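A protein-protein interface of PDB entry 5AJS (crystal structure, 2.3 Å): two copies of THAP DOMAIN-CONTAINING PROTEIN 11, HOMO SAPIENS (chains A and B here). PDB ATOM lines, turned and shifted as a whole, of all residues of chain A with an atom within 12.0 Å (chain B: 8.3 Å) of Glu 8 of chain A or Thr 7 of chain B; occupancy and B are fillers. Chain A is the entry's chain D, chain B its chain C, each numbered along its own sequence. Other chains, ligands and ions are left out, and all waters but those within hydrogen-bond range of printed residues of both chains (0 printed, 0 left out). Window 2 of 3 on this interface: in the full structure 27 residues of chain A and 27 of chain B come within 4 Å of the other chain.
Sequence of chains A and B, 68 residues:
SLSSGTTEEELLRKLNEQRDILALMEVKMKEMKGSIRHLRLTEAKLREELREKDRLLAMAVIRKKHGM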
ATOM      1  N   GLY A   5     -36.864  -6.004  15.479  1.00  0.00           N
ATOM      2  CA  GLY A   5     -36.490  -6.201  16.911  1.00  0.00           C
ATOM      3  C   GLY A   5     -35.112  -6.824  17.065  1.00  0.00           C
ATOM      4  O   GLY A   5     -34.662  -7.572  16.186  1.00  0.00           O
ATOM      5  N   THR A   6     -34.440  -6.515  18.178  1.00  0.00           N
ATOM      6  CA  THR A   6     -33.100  -7.064  18.472  1.00  0.00           C
ATOM      7  C   THR A   6     -33.210  -8.591  18.736  1.00  0.00           C
ATOM      8  O   THR A   6     -34.254  -9.072  19.186  1.00  0.00           O
ATOM      9  CB  THR A   6     -32.383  -6.280  19.616  1.00  0.00           C
ATOM     10  OG1 THR A   6     -33.349  -5.737  20.522  1.00  0.00           O
ATOM     11  CG2 THR A   6     -31.569  -5.102  19.063  1.00  0.00           C
ATOM     12  N   THR A   7     -32.142  -9.337  18.431  1.00  0.00           N
ATOM     13  CA  THR A   7     -32.221 -10.797  18.155  1.00  0.00           C
ATOM     14  C   THR A   7     -32.137 -11.702  19.406  1.00  0.00           C
ATOM     15  O   THR A   7     -32.238 -11.200  20.530  1.00  0.00           O
ATOM     16  CB  THR A   7     -31.138 -11.216  17.129  1.00  0.00           C
ATOM     17  N   GLU A   8     -31.976 -13.021  19.205  1.00  0.00           N
ATOM     18  CA  GLU A   8     -31.997 -14.006  20.310  1.00  0.00           C
ATOM     19  C   GLU A   8     -30.984 -13.673  21.412  1.00  0.00           C
ATOM     20  O   GLU A   8     -29.793 -13.469  21.136  1.00  0.00           O
ATOM     21  CB  GLU A   8     -31.753 -15.439  19.802  1.00  0.00           C
ATOM     22  N   GLU A   9     -31.466 -13.619  22.659  1.00  0.00           N
ATOM     23  CA  GLU A   9     -30.632 -13.224  23.796  1.00  0.00           C
ATOM     24  C   GLU A   9     -29.574 -14.281  24.106  1.00  0.00           C
ATOM     25  O   GLU A   9     -28.590 -13.984  24.779  1.00  0.00           O
ATOM     26  CB  GLU A   9     -31.482 -12.918  25.040  1.00  0.00           C
ATOM     27  N   GLU A  10     -29.773 -15.505  23.611  1.00  0.00           N
ATOM     28  CA  GLU A  10     -28.816 -16.597  23.828  1.00  0.00           C
ATOM     29  C   GLU A  10     -27.558 -16.344  22.993  1.00  0.00           C
ATOM     30  O   GLU A  10     -26.478 -16.079  23.542  1.00  0.00           O
ATOM     31  CB  GLU A  10     -29.451 -17.951  23.468  1.00  0.00           C
ATOM     32  N   LEU A  11     -27.721 -16.416  21.669  1.00  0.00           N
ATOM     33  CA  LEU A  11     -26.718 -15.976  20.716  1.00  0.00           C
ATOM     34  C   LEU A  11     -25.860 -14.856  21.256  1.00  0.00           C
ATOM     35  O   LEU A  11     -24.636 -15.012  21.380  1.00  0.00           O
ATOM     36  CB  LEU A  11     -27.395 -15.481  19.439  1.00  0.00           C
ATOM     37  CG  LEU A  11     -27.746 -16.587  18.441  1.00  0.00           C
ATOM     38  CD1 LEU A  11     -28.708 -16.075  17.385  1.00  0.00           C
ATOM     39  CD2 LEU A  11     -26.498 -17.145  17.778  1.00  0.00           C
ATOM     40  N   LEU A  12     -26.544 -13.754  21.588  1.00  0.00           N
ATOM     41  CA  LEU A  12     -25.950 -12.527  22.112  1.00  0.00           C
ATOM     42  C   LEU A  12     -25.121 -12.731  23.388  1.00  0.00           C
ATOM     43  O   LEU A  12     -24.012 -12.164  23.496  1.00  0.00           O
ATOM     44  CB  LEU A  12     -27.035 -11.458  22.346  1.00  0.00           C
ATOM     45  CG  LEU A  12     -27.640 -10.922  21.037  1.00  0.00           C
ATOM     46  CD1 LEU A  12     -29.062 -10.409  21.229  1.00  0.00           C
ATOM     47  CD2 LEU A  12     -26.773  -9.844  20.395  1.00  0.00           C
ATOM     48  N   ARG A  13     -25.627 -13.529  24.337  1.00  0.00           N
ATOM     49  CA  ARG A  13     -24.867 -13.813  25.544  1.00  0.00           C
ATOM     50  C   ARG A  13     -23.582 -14.544  25.135  1.00  0.00           C
ATOM     51  O   ARG A  13     -22.505 -14.352  25.718  1.00  0.00           O
ATOM     52  CB  ARG A  13     -25.674 -14.682  26.512  1.00  0.00           C
ATOM     53  N   LYS A  14     -23.725 -15.379  24.111  1.00  0.00           N
ATOM     54  CA  LYS A  14     -22.631 -16.156  23.575  1.00  0.00           C
ATOM     55  C   LYS A  14     -21.577 -15.284  22.889  1.00  0.00           C
ATOM     56  O   LYS A  14     -20.378 -15.535  23.040  1.00  0.00           O
ATOM     57  CB  LYS A  14     -23.170 -17.220  22.606  1.00  0.00           C
ATOM     58  N   LEU A  15     -22.027 -14.265  22.152  1.00  0.00           N
ATOM     59  CA  LEU A  15     -21.122 -13.398  21.416  1.00  0.00           C
ATOM     60  C   LEU A  15     -20.266 -12.653  22.386  1.00  0.00           C
ATOM     61  O   LEU A  15     -19.011 -12.521  22.195  1.00  0.00           O
ATOM     62  CB  LEU A  15     -21.891 -12.420  20.506  1.00  0.00           C
ATOM     63  CG  LEU A  15     -22.437 -13.124  19.274  1.00  0.00           C
ATOM     64  CD1 LEU A  15     -23.612 -12.374  18.658  1.00  0.00           C
ATOM     65  CD2 LEU A  15     -21.320 -13.324  18.274  1.00  0.00           C
ATOM     66  N   ASN A  16     -20.933 -12.208  23.454  1.00  0.00           N
ATOM     67  CA  ASN A  16     -20.251 -11.403  24.456  1.00  0.00           C
ATOM     68  C   ASN A  16     -19.294 -12.217  25.264  1.00  0.00           C
ATOM     69  O   ASN A  16     -18.186 -11.730  25.601  1.00  0.00           O
ATOM     70  CB  ASN A  16     -21.223 -10.654  25.344  1.00  0.00           C
ATOM     71  CG  ASN A  16     -21.835  -9.446  24.640  1.00  0.00           C
ATOM     72  OD1 ASN A  16     -21.243  -8.358  24.612  1.00  0.00           O
ATOM     73  ND2 ASN A  16     -23.005  -9.634  24.048  1.00  0.00           N
ATOM     74  N   GLU A  17     -19.684 -13.457  25.532  1.00  0.00           N
ATOM     75  CA  GLU A  17     -18.803 -14.362  26.285  1.00  0.00           C
ATOM     76  C   GLU A  17     -17.472 -14.582  25.562  1.00  0.00           C
ATOM     77  O   GLU A  17     -16.391 -14.429  26.135  1.00  0.00           O
ATOM     78  CB  GLU A  17     -19.481 -15.706  26.470  1.00  0.00           C
ATOM     79  CG  GLU A  17     -18.479 -16.796  26.792  1.00  0.00           C
ATOM     80  CD  GLU A  17     -19.087 -18.066  27.348  1.00  0.00           C
ATOM     81  OE1 GLU A  17     -20.331 -18.298  27.155  1.00  0.00           O
ATOM     82  OE2 GLU A  17     -18.281 -18.814  27.982  1.00  0.00           O
ATOM     83  N   THR B   7     -32.425 -17.008  16.732  1.00  0.00           N
ATOM     84  CA  THR B   7     -31.694 -17.916  15.786  1.00  0.00           C
ATOM     85  C   THR B   7     -31.271 -17.196  14.477  1.00  0.00           C
ATOM     86  O   THR B   7     -31.320 -17.788  13.393  1.00  0.00           O
ATOM     87  CB  THR B   7     -32.521 -19.191  15.478  1.00  0.00           C
ATOM     88  N   GLU B   8     -30.827 -15.939  14.600  1.00  0.00           N
ATOM     89  CA  GLU B   8     -30.450 -15.079  13.452  1.00  0.00           C
ATOM     90  C   GLU B   8     -29.158 -15.525  12.723  1.00  0.00           C
ATOM     91  O   GLU B   8     -28.106 -15.761  13.354  1.00  0.00           O
ATOM     92  CB  GLU B   8     -30.314 -13.622  13.914  1.00  0.00           C
ATOM     93  N   GLU B   9     -29.250 -15.609  11.390  1.00  0.00           N
ATOM     94  CA  GLU B   9     -28.194 -16.192  10.544  1.00  0.00           C
ATOM     95  C   GLU B   9     -26.842 -15.521  10.697  1.00  0.00           C
ATOM     96  O   GLU B   9     -25.825 -16.210  10.714  1.00  0.00           O
ATOM     97  CB  GLU B   9     -28.578 -16.133   9.062  1.00  0.00           C
ATOM     98  N   GLU B  10     -26.843 -14.184  10.789  1.00  0.00           N
ATOM     99  CA  GLU B  10     -25.605 -13.371  10.829  1.00  0.00           C
ATOM    100  C   GLU B  10     -24.943 -13.352  12.205  1.00  0.00           C
ATOM    101  O   GLU B  10     -23.734 -13.155  12.262  1.00  0.00           O
ATOM    102  CB  GLU B  10     -25.850 -11.914  10.389  1.00  0.00           C
ATOM    103  N   LEU B  11     -25.733 -13.530  13.280  1.00  0.00           N
ATOM    104  CA  LEU B  11     -25.207 -13.664  14.655  1.00  0.00           C
ATOM    105  C   LEU B  11     -24.391 -14.940  14.804  1.00  0.00           C
ATOM    106  O   LEU B  11     -23.292 -14.918  15.329  1.00  0.00           O
ATOM    107  CB  LEU B  11     -26.339 -13.689  15.693  1.00  0.00           C
ATOM    108  CG  LEU B  11     -26.995 -12.353  16.103  1.00  0.00           C
ATOM    109  CD1 LEU B  11     -27.589 -12.430  17.521  1.00  0.00           C
ATOM    110  CD2 LEU B  11     -26.029 -11.179  16.019  1.00  0.00           C
ATOM    111  N   LEU B  12     -24.977 -16.041  14.343  1.00  0.00           N
ATOM    112  CA  LEU B  12     -24.328 -17.346  14.246  1.00  0.00           C
ATOM    113  C   LEU B  12     -23.051 -17.307  13.439  1.00  0.00           C
ATOM    114  O   LEU B  12     -22.077 -17.960  13.803  1.00  0.00           O
ATOM    115  CB  LEU B  12     -25.254 -18.353  13.567  1.00  0.00           C
ATOM    116  CG  LEU B  12     -26.530 -18.688  14.336  1.00  0.00           C
ATOM    117  CD1 LEU B  12     -27.710 -18.947  13.402  1.00  0.00           C
ATOM    118  CD2 LEU B  12     -26.277 -19.864  15.278  1.00  0.00           C
ATOM    119  N   LEU B  15     -20.662 -15.688  15.644  1.00  0.00           N
ATOM    120  CA  LEU B  15     -20.155 -16.625  16.629  1.00  0.00           C
ATOM    121  C   LEU B  15     -18.992 -17.417  16.079  1.00  0.00           C
ATOM    122  O   LEU B  15     -17.960 -17.591  16.790  1.00  0.00           O
ATOM    123  CB  LEU B  15     -21.255 -17.574  17.095  1.00  0.00           C
ATOM    124  CG  LEU B  15     -22.103 -17.028  18.249  1.00  0.00           C
ATOM    125  CD1 LEU B  15     -23.413 -17.791  18.403  1.00  0.00           C
ATOM    126  CD2 LEU B  15     -21.331 -17.045  19.556  1.00  0.00           C
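Printed residues of chain A that touch a printed residue of chain B: Thr 7, Glu 8, Leu 11, Leu 12, Lys 14 and Leu 15. Hydrophobic or aromatic side chains of chain A that line the printed part of chain B: Leu 11, Leu 12 and Leu 15. Hydrophobic or aromatic side chains of chain B within 4 Å of the printed part of chain A: Leu 11, Leu 12 and Leu 15. Among the printed residues, no Asp or Glu carboxylate lies within 4 Å of a Lys or Arg side-chain nitrogen of the other chain.
O of Leu 12 of chain A sits at hydrogen-bond distance from ND2 of Asn 16 of chain A (2.8 Å).
CD1 of Leu 11 of chain B touches CB of Thr 7 of chain A (3.8 Å). Thr 7 of chain B touches Glu 8 of chain A. CA of Thr 7 of chain B touches CD1 of Leu 11 of chain A (3.9 Å). Glu 8 of chain B touches Leu 11 of chain A (N to CD1, 3.5 Å). Leu 11 of chain B touches Leu 11 of chain A. Leu 11 of chain A touches Leu 12 of chain B. CG of Leu 12 of chain A touches CD1 of Leu 11 of chain B (3.8 Å). Lys 14 of chain A touches Leu 15 of chain B (CB to CD2, 3.6 Å). CD1 of Leu 15 of chain A touches CD2 of Leu 11 of chain B (3.8 Å). N of Leu 15 of chain B touches CD2 of Leu 15 of chain A, at 3.6 Å.
Glu 8 of chain A touches Thr 7 of chain B, but with the chains exchanged Thr 7 of chain A does not touch Glu 8 of chain B (4.1 Å). Leu 11 of chain B touches its own counterpart, Leu 11 of chain A. Leu 11 of chain A touches Leu 15 of chain B, and with the chains exchanged Leu 15 of chain A touches Leu 11 of chain B. Leu 15 of chain B touches its own counterpart, Leu 15 of chain A.
Of the printed residues of chain B, Glu 8 of chain A touches Thr 7 (3.5 Å). Thr 7 of chain B touches just these residues of chain A: Glu 8 and Leu 11. Glu 8 of chain B touches just one residue of chain A: Leu 11 (3.5 Å). Of the printed residues of chain A, Leu 12 of chain B touches Leu 11 (3.7 Å). Printed residues of chain A within 4 Å of Leu 15 of chain B: Leu 11 (3.2 Å), Lys 14 (3.6 Å) and Leu 15 (3.6 Å). Of the printed residues of chain B, Lys 14 of chain A touches Leu 15. Of the printed residues of chain B, Leu 12 of chain A touches Leu 11. Printed residues of chain B within 4 Å of Leu 15 of chain A: Leu 11 and Leu 15. The nearest residue of chain B that does not touch Glu 8 of chain A is Leu 11 of chain B (4.4 Å). The nearest residue of chain A that does not touch Thr 7 of chain B is Thr 7 of chain A (5.9 Å).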
